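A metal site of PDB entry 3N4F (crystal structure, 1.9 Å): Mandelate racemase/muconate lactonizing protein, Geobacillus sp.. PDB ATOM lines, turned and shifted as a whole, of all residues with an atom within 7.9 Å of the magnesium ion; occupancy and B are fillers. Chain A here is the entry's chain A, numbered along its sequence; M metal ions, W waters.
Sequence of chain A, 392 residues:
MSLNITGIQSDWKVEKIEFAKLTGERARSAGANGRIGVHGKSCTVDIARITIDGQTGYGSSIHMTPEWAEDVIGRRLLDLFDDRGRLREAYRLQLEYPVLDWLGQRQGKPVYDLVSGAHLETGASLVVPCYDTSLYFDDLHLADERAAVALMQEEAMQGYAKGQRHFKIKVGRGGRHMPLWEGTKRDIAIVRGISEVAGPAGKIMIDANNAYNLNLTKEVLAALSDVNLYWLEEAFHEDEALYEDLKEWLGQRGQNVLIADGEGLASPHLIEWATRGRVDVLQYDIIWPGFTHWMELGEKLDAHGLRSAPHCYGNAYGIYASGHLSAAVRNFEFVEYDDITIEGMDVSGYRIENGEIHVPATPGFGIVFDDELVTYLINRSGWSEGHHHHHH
The backbone NH of Asn 209 lies within hydrogen-bond range of the side-chain carboxylate of Asp 207, at 2.8 Å. OE1 of Glu 233 lies within salt-bridge range of NZ of Lys 168 (2.9 Å). NZ of Lys 170 lies within hydrogen-bond range of OD1 of Asn 209, at 2.8 Å. N of Glu 233 sits at hydrogen-bond distance from O of Ile 206 (2.9 Å). The side-chain carboxylate of Glu 233 lies within hydrogen-bond range of the side-chain amide nitrogen of Gln 283 (2.9 Å). OE1 of Glu 233 is in hydrogen-bond range of NE1 of Trp 231 (3.2 Å). O of Glu 233 lies within hydrogen-bond range of N of Ala 208 (3.2 Å). OD2 of Asp 207 sits close to NZ of Lys 170, at 3.0 Å.
Lys 170 touches the magnesium ion (NZ to MG, 3.9 Å). Of the 24 residues printed, 4 come within 4 Å of the magnesium ion.
The magnesium ion is bound by OE2 of Glu 233 (2.0 Å), water W3 (2.0 Å), water W1 (2.1 Å), water W2 (2.1 Å), OD2 of Asp 207 (2.1 Å) and OE2 of Glu 263 (2.2 Å). The magnesium ion has six donor atoms within binding distance.
Water W3 lies within hydrogen-bond range of the side-chain carboxylate of Glu 263 (2.6 Å), the side-chain amino group of Lys 170 (3.0 Å) and the side-chain amide nitrogen of Asn 209 (3.1 Å). Water W2 lies within hydrogen-bond range of the side-chain amino group (NZ) of Lys 168 and the side-chain carboxylate (OE2) of Glu 336. Water W1 lies within hydrogen-bond range of the side-chain carboxylate of Glu 234, the side-chain carboxylate of Asp 207 and the side-chain amide nitrogen of Asn 209.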
ATOM      1  N   ASN A  33      23.191  -4.155  17.671  1.00  0.00           N
ATOM      2  CA  ASN A  33      22.064  -5.013  17.455  1.00  0.00           C
ATOM      3  C   ASN A  33      22.201  -5.436  15.997  1.00  0.00           C
ATOM      4  O   ASN A  33      23.200  -5.116  15.348  1.00  0.00           O
ATOM      5  CB  ASN A  33      20.722  -4.297  17.788  1.00  0.00           C
ATOM      6  CG  ASN A  33      20.318  -3.229  16.754  1.00  0.00           C
ATOM      7  OD1 ASN A  33      20.887  -3.125  15.663  1.00  0.00           O
ATOM      8  ND2 ASN A  33      19.274  -2.442  17.105  1.00  0.00           N
ATOM      9  N   TYR A 131      10.242  -7.695  31.074  1.00  0.00           N
ATOM     10  CA  TYR A 131      11.411  -8.457  30.672  1.00  0.00           C
ATOM     11  C   TYR A 131      12.620  -7.535  30.538  1.00  0.00           C
ATOM     12  O   TYR A 131      12.486  -6.324  30.334  1.00  0.00           O
ATOM     13  CB  TYR A 131      11.170  -9.233  29.385  1.00  0.00           C
ATOM     14  CG  TYR A 131      10.906  -8.382  28.173  1.00  0.00           C
ATOM     15  CD1 TYR A 131      11.952  -7.806  27.450  1.00  0.00           C
ATOM     16  CD2 TYR A 131       9.606  -8.158  27.733  1.00  0.00           C
ATOM     17  CE1 TYR A 131      11.704  -7.023  26.319  1.00  0.00           C
ATOM     18  CE2 TYR A 131       9.344  -7.371  26.604  1.00  0.00           C
ATOM     19  CZ  TYR A 131      10.400  -6.810  25.923  1.00  0.00           C
ATOM     20  OH  TYR A 131      10.161  -6.056  24.805  1.00  0.00           O
ATOM     21  N   THR A 133      15.434  -6.116  28.530  1.00  0.00           N
ATOM     22  CA  THR A 133      15.668  -5.890  27.084  1.00  0.00           C
ATOM     23  C   THR A 133      17.130  -5.561  26.751  1.00  0.00           C
ATOM     24  O   THR A 133      17.499  -5.358  25.581  1.00  0.00           O
ATOM     25  CB  THR A 133      14.710  -4.774  26.541  1.00  0.00           C
ATOM     26  OG1 THR A 133      14.607  -4.850  25.104  1.00  0.00           O
ATOM     27  CG2 THR A 133      15.188  -3.384  26.914  1.00  0.00           C
ATOM     28  N   TYR A 136      22.167  -6.878  24.495  1.00  0.00           N
ATOM     29  CA  TYR A 136      22.634  -6.498  23.159  1.00  0.00           C
ATOM     30  C   TYR A 136      23.838  -7.334  22.732  1.00  0.00           C
ATOM     31  O   TYR A 136      24.255  -8.223  23.483  1.00  0.00           O
ATOM     32  CB  TYR A 136      22.903  -4.985  23.120  1.00  0.00           C
ATOM     33  CG  TYR A 136      21.633  -4.187  22.874  1.00  0.00           C
ATOM     34  CD1 TYR A 136      20.541  -4.283  23.752  1.00  0.00           C
ATOM     35  CD2 TYR A 136      21.494  -3.387  21.738  1.00  0.00           C
ATOM     36  CE1 TYR A 136      19.343  -3.571  23.506  1.00  0.00           C
ATOM     37  CE2 TYR A 136      20.310  -2.678  21.489  1.00  0.00           C
ATOM     38  CZ  TYR A 136      19.244  -2.782  22.363  1.00  0.00           C
ATOM     39  OH  TYR A 136      18.066  -2.094  22.096  1.00  0.00           O
ATOM     40  N   LYS A 168      14.877 -10.662  26.784  1.00  0.00           N
ATOM     41  CA  LYS A 168      14.829 -10.533  25.321  1.00  0.00           C
ATOM     42  C   LYS A 168      16.251 -10.363  24.838  1.00  0.00           C
ATOM     43  O   LYS A 168      16.974  -9.442  25.252  1.00  0.00           O
ATOM     44  CB  LYS A 168      13.985  -9.359  24.837  1.00  0.00           C
ATOM     45  CG  LYS A 168      13.751  -9.343  23.298  1.00  0.00           C
ATOM     46  CD  LYS A 168      13.419  -7.953  22.742  1.00  0.00           C
ATOM     47  CE  LYS A 168      12.002  -7.566  22.961  1.00  0.00           C
ATOM     48  NZ  LYS A 168      11.746  -6.149  22.509  1.00  0.00           N
ATOM     49  N   LYS A 170      19.075  -9.984  21.869  1.00  0.00           N
ATOM     50  CA  LYS A 170      19.328  -9.595  20.473  1.00  0.00           C
ATOM     51  C   LYS A 170      20.031 -10.706  19.732  1.00  0.00           C
ATOM     52  O   LYS A 170      21.010 -11.302  20.221  1.00  0.00           O
ATOM     53  CB  LYS A 170      20.137  -8.301  20.390  1.00  0.00           C
ATOM     54  CG  LYS A 170      19.456  -7.065  21.043  1.00  0.00           C
ATOM     55  CD  LYS A 170      18.140  -6.724  20.347  1.00  0.00           C
ATOM     56  CE  LYS A 170      17.682  -5.305  20.673  1.00  0.00           C
ATOM     57  NZ  LYS A 170      16.624  -4.859  19.729  1.00  0.00           N
ATOM     58  N   ILE A 206      13.508 -13.492  21.407  1.00  0.00           N
ATOM     59  CA  ILE A 206      14.633 -13.143  20.562  1.00  0.00           C
ATOM     60  C   ILE A 206      14.219 -12.068  19.549  1.00  0.00           C
ATOM     61  O   ILE A 206      13.107 -12.087  18.998  1.00  0.00           O
ATOM     62  CB  ILE A 206      15.286 -14.384  19.884  1.00  0.00           C
ATOM     63  CG1 ILE A 206      14.271 -15.162  19.020  1.00  0.00           C
ATOM     64  CG2 ILE A 206      15.873 -15.307  20.968  1.00  0.00           C
ATOM     65  CD1 ILE A 206      14.882 -16.320  18.202  1.00  0.00           C
ATOM     66  N   ASP A 207      15.120 -11.123  19.310  1.00  0.00           N
ATOM     67  CA  ASP A 207      14.835 -10.012  18.430  1.00  0.00           C
ATOM     68  C   ASP A 207      15.962  -9.902  17.418  1.00  0.00           C
ATOM     69  O   ASP A 207      17.113  -9.639  17.774  1.00  0.00           O
ATOM     70  CB  ASP A 207      14.713  -8.752  19.283  1.00  0.00           C
ATOM     71  CG  ASP A 207      14.477  -7.482  18.469  1.00  0.00           C
ATOM     72  OD1 ASP A 207      14.544  -7.473  17.199  1.00  0.00           O
ATOM     73  OD2 ASP A 207      14.215  -6.465  19.114  1.00  0.00           O
ATOM     74  N   ALA A 208      15.636 -10.100  16.153  1.00  0.00           N
ATOM     75  CA  ALA A 208      16.653 -10.068  15.105  1.00  0.00           C
ATOM     76  C   ALA A 208      16.863  -8.726  14.444  1.00  0.00           C
ATOM     77  O   ALA A 208      17.706  -8.626  13.535  1.00  0.00           O
ATOM     78  CB  ALA A 208      16.349 -11.113  14.045  1.00  0.00           C
ATOM     79  N   ASN A 209      16.108  -7.709  14.840  1.00  0.00           N
ATOM     80  CA  ASN A 209      16.152  -6.431  14.142  1.00  0.00           C
ATOM     81  C   ASN A 209      16.236  -6.564  12.624  1.00  0.00           C
ATOM     82  O   ASN A 209      17.050  -5.887  11.993  1.00  0.00           O
ATOM     83  CB  ASN A 209      17.276  -5.546  14.706  1.00  0.00           C
ATOM     84  CG  ASN A 209      16.900  -4.967  16.062  1.00  0.00           C
ATOM     85  OD1 ASN A 209      17.347  -5.441  17.098  1.00  0.00           O
ATOM     86  ND2 ASN A 209      15.985  -3.995  16.054  1.00  0.00           N
ATOM     87  N   ASN A 210      15.414  -7.469  12.073  1.00  0.00           N
ATOM     88  CA  ASN A 210      15.249  -7.698  10.613  1.00  0.00           C
ATOM     89  C   ASN A 210      16.429  -8.357   9.859  1.00  0.00           C
ATOM     90  O   ASN A 210      16.434  -8.418   8.604  1.00  0.00           O
ATOM     91  CB  ASN A 210      14.815  -6.399   9.908  1.00  0.00           C
ATOM     92  CG  ASN A 210      13.393  -5.984  10.279  1.00  0.00           C
ATOM     93  OD1 ASN A 210      12.606  -6.793  10.750  1.00  0.00           O
ATOM     94  ND2 ASN A 210      13.074  -4.720  10.074  1.00  0.00           N
ATOM     95  N   TRP A 231       8.509 -15.414  22.281  1.00  0.00           N
ATOM     96  CA  TRP A 231       8.240 -14.792  20.976  1.00  0.00           C
ATOM     97  C   TRP A 231       9.478 -14.526  20.151  1.00  0.00           C
ATOM     98  O   TRP A 231      10.600 -14.421  20.696  1.00  0.00           O
ATOM     99  CB  TRP A 231       7.303 -13.538  21.068  1.00  0.00           C
ATOM    100  CG  TRP A 231       7.923 -12.203  21.452  1.00  0.00           C
ATOM    101  CD1 TRP A 231       9.082 -11.630  20.974  1.00  0.00           C
ATOM    102  CD2 TRP A 231       7.363 -11.243  22.376  1.00  0.00           C
ATOM    103  NE1 TRP A 231       9.267 -10.390  21.549  1.00  0.00           N
ATOM    104  CE2 TRP A 231       8.235 -10.138  22.416  1.00  0.00           C
ATOM    105  CE3 TRP A 231       6.203 -11.221  23.175  1.00  0.00           C
ATOM    106  CZ2 TRP A 231       8.004  -9.013  23.243  1.00  0.00           C
ATOM    107  CZ3 TRP A 231       5.969 -10.098  23.992  1.00  0.00           C
ATOM    108  CH2 TRP A 231       6.861  -9.017  24.011  1.00  0.00           C
ATOM    109  N   GLU A 233      10.700 -11.689  17.381  1.00  0.00           N
ATOM    110  CA  GLU A 233      10.386 -10.299  17.080  1.00  0.00           C
ATOM    111  C   GLU A 233      11.256  -9.860  15.920  1.00  0.00           C
ATOM    112  O   GLU A 233      12.486 -10.007  15.968  1.00  0.00           O
ATOM    113  CB  GLU A 233      10.681  -9.459  18.313  1.00  0.00           C
ATOM    114  CG  GLU A 233      10.818  -7.953  18.064  1.00  0.00           C
ATOM    115  CD  GLU A 233      10.900  -7.166  19.360  1.00  0.00           C
ATOM    116  OE1 GLU A 233      10.562  -7.727  20.431  1.00  0.00           O
ATOM    117  OE2 GLU A 233      11.274  -5.976  19.293  1.00  0.00           O
ATOM    118  N   GLU A 234      10.606  -9.319  14.894  1.00  0.00           N
ATOM    119  CA  GLU A 234      11.286  -8.773  13.703  1.00  0.00           C
ATOM    120  C   GLU A 234      12.394  -9.681  13.184  1.00  0.00           C
ATOM    121  O   GLU A 234      13.550  -9.254  13.043  1.00  0.00           O
ATOM    122  CB  GLU A 234      11.844  -7.364  13.984  1.00  0.00           C
ATOM    123  CG  GLU A 234      10.768  -6.307  14.305  1.00  0.00           C
ATOM    124  CD  GLU A 234      11.199  -4.889  13.958  1.00  0.00           C
ATOM    125  OE1 GLU A 234      12.272  -4.444  14.433  1.00  0.00           O
ATOM    126  OE2 GLU A 234      10.445  -4.197  13.218  1.00  0.00           O
ATOM    127  N   ALA A 260       6.079 -11.336  16.888  1.00  0.00           N
ATOM    128  CA  ALA A 260       5.947  -9.951  17.359  1.00  0.00           C
ATOM    129  C   ALA A 260       6.526  -9.015  16.329  1.00  0.00           C
ATOM    130  O   ALA A 260       7.583  -9.295  15.762  1.00  0.00           O
ATOM    131  CB  ALA A 260       6.673  -9.758  18.718  1.00  0.00           C
ATOM    132  N   ASP A 261       5.839  -7.898  16.092  1.00  0.00           N
ATOM    133  CA  ASP A 261       6.385  -6.918  15.154  1.00  0.00           C
ATOM    134  C   ASP A 261       5.695  -5.582  15.387  1.00  0.00           C
ATOM    135  O   ASP A 261       4.762  -5.496  16.190  1.00  0.00           O
ATOM    136  CB  ASP A 261       6.164  -7.411  13.721  1.00  0.00           C
ATOM    137  CG  ASP A 261       7.315  -7.052  12.785  1.00  0.00           C
ATOM    138  OD1 ASP A 261       7.798  -5.907  12.837  1.00  0.00           O
ATOM    139  OD2 ASP A 261       7.743  -7.931  12.009  1.00  0.00           O
ATOM    140  N   GLY A 262       6.167  -4.539  14.713  1.00  0.00           N
ATOM    141  CA  GLY A 262       5.485  -3.267  14.738  1.00  0.00           C
ATOM    142  C   GLY A 262       6.269  -2.024  15.093  1.00  0.00           C
ATOM    143  O   GLY A 262       5.780  -0.916  14.900  1.00  0.00           O
ATOM    144  N   GLU A 263       7.496  -2.183  15.610  1.00  0.00           N
ATOM    145  CA  GLU A 263       8.295  -0.991  15.920  1.00  0.00           C
ATOM    146  C   GLU A 263       8.789  -0.291  14.647  1.00  0.00           C
ATOM    147  O   GLU A 263       8.667  -0.826  13.533  1.00  0.00           O
ATOM    148  CB  GLU A 263       9.435  -1.317  16.888  1.00  0.00           C
ATOM    149  CG  GLU A 263      10.599  -2.003  16.224  1.00  0.00           C
ATOM    150  CD  GLU A 263      11.681  -2.363  17.211  1.00  0.00           C
ATOM    151  OE1 GLU A 263      12.767  -1.755  17.105  1.00  0.00           O
ATOM    152  OE2 GLU A 263      11.449  -3.244  18.076  1.00  0.00           O
ATOM    153  N   GLY A 264       9.311   0.928  14.803  1.00  0.00           N
ATOM    154  CA  GLY A 264       9.912   1.663  13.668  1.00  0.00           C
ATOM    155  C   GLY A 264       8.966   1.967  12.518  1.00  0.00           C
ATOM    156  O   GLY A 264       7.803   2.305  12.734  1.00  0.00           O
ATOM    157  N   GLN A 283       3.747  -4.025  18.478  1.00  0.00           N
ATOM    158  CA  GLN A 283       4.808  -3.352  19.258  1.00  0.00           C
ATOM    159  C   GLN A 283       5.072  -1.879  18.936  1.00  0.00           C
ATOM    160  O   GLN A 283       6.209  -1.391  19.079  1.00  0.00           O
ATOM    161  CB  GLN A 283       6.125  -4.127  19.159  1.00  0.00           C
ATOM    162  CG  GLN A 283       6.037  -5.534  19.671  1.00  0.00           C
ATOM    163  CD  GLN A 283       7.327  -6.270  19.518  1.00  0.00           C
ATOM    164  OE1 GLN A 283       7.810  -6.485  18.407  1.00  0.00           O
ATOM    165  NE2 GLN A 283       7.901  -6.689  20.642  1.00  0.00           N
ATOM    166  N   HIS A 311       6.710  -0.964  22.341  1.00  0.00           N
ATOM    167  CA  HIS A 311       8.140  -0.768  22.277  1.00  0.00           C
ATOM    168  C   HIS A 311       8.552   0.357  23.218  1.00  0.00           C
ATOM    169  O   HIS A 311       7.893   1.414  23.307  1.00  0.00           O
ATOM    170  CB  HIS A 311       8.596  -0.434  20.859  1.00  0.00           C
ATOM    171  CG  HIS A 311      10.045  -0.042  20.756  1.00  0.00           C
ATOM    172  ND1 HIS A 311      10.461   1.272  20.824  1.00  0.00           N
ATOM    173  CD2 HIS A 311      11.170  -0.775  20.534  1.00  0.00           C
ATOM    174  CE1 HIS A 311      11.779   1.330  20.683  1.00  0.00           C
ATOM    175  NE2 HIS A 311      12.222   0.095  20.494  1.00  0.00           N
ATOM    176  N   CYS A 312       9.627   0.120  23.946  1.00  0.00           N
ATOM    177  CA  CYS A 312      10.247   1.139  24.748  1.00  0.00           C
ATOM    178  C   CYS A 312      11.750   0.893  24.724  1.00  0.00           C
ATOM    179  O   CYS A 312      12.243  -0.104  25.209  1.00  0.00           O
ATOM    180  CB  CYS A 312       9.728   1.071  26.184  1.00  0.00           C
ATOM    181  SG  CYS A 312      10.225   2.511  27.094  1.00  0.00           S
ATOM    182  N   TYR A 313      12.477   1.810  24.101  1.00  0.00           N
ATOM    183  CA  TYR A 313      13.915   1.809  24.163  1.00  0.00           C
ATOM    184  C   TYR A 313      14.385   3.202  23.780  1.00  0.00           C
ATOM    185  O   TYR A 313      13.930   3.754  22.785  1.00  0.00           O
ATOM    186  CB  TYR A 313      14.551   0.753  23.229  1.00  0.00           C
ATOM    187  CG  TYR A 313      15.989   0.480  23.638  1.00  0.00           C
ATOM    188  CD1 TYR A 313      16.278  -0.376  24.691  1.00  0.00           C
ATOM    189  CD2 TYR A 313      17.057   1.155  23.017  1.00  0.00           C
ATOM    190  CE1 TYR A 313      17.605  -0.622  25.098  1.00  0.00           C
ATOM    191  CE2 TYR A 313      18.387   0.923  23.421  1.00  0.00           C
ATOM    192  CZ  TYR A 313      18.633   0.030  24.458  1.00  0.00           C
ATOM    193  OH  TYR A 313      19.911  -0.209  24.875  1.00  0.00           O
ATOM    194  N   GLU A 336       8.760  -3.505  28.572  1.00  0.00           N
ATOM    195  CA  GLU A 336      10.125  -3.692  28.091  1.00  0.00           C
ATOM    196  C   GLU A 336      11.032  -2.871  28.991  1.00  0.00           C
ATOM    197  O   GLU A 336      10.972  -1.642  28.987  1.00  0.00           O
ATOM    198  CB  GLU A 336      10.209  -3.208  26.631  1.00  0.00           C
ATOM    199  CG  GLU A 336      11.590  -3.346  26.024  1.00  0.00           C
ATOM    200  CD  GLU A 336      11.608  -3.205  24.493  1.00  0.00           C
ATOM    201  OE1 GLU A 336      10.645  -2.698  23.891  1.00  0.00           O
ATOM    202  OE2 GLU A 336      12.619  -3.618  23.876  1.00  0.00           O
HETATM  203 MG    MG M   1      12.864  -4.850  18.764  1.00  0.00          MG
HETATM  204  O   HOH W   1      12.940  -5.314  16.766  1.00  0.00           O
HETATM  205  O   HOH W   2      12.966  -4.178  20.760  1.00  0.00           O
HETATM  206  O   HOH W   3      14.250  -3.375  18.569  1.00  0.00           O
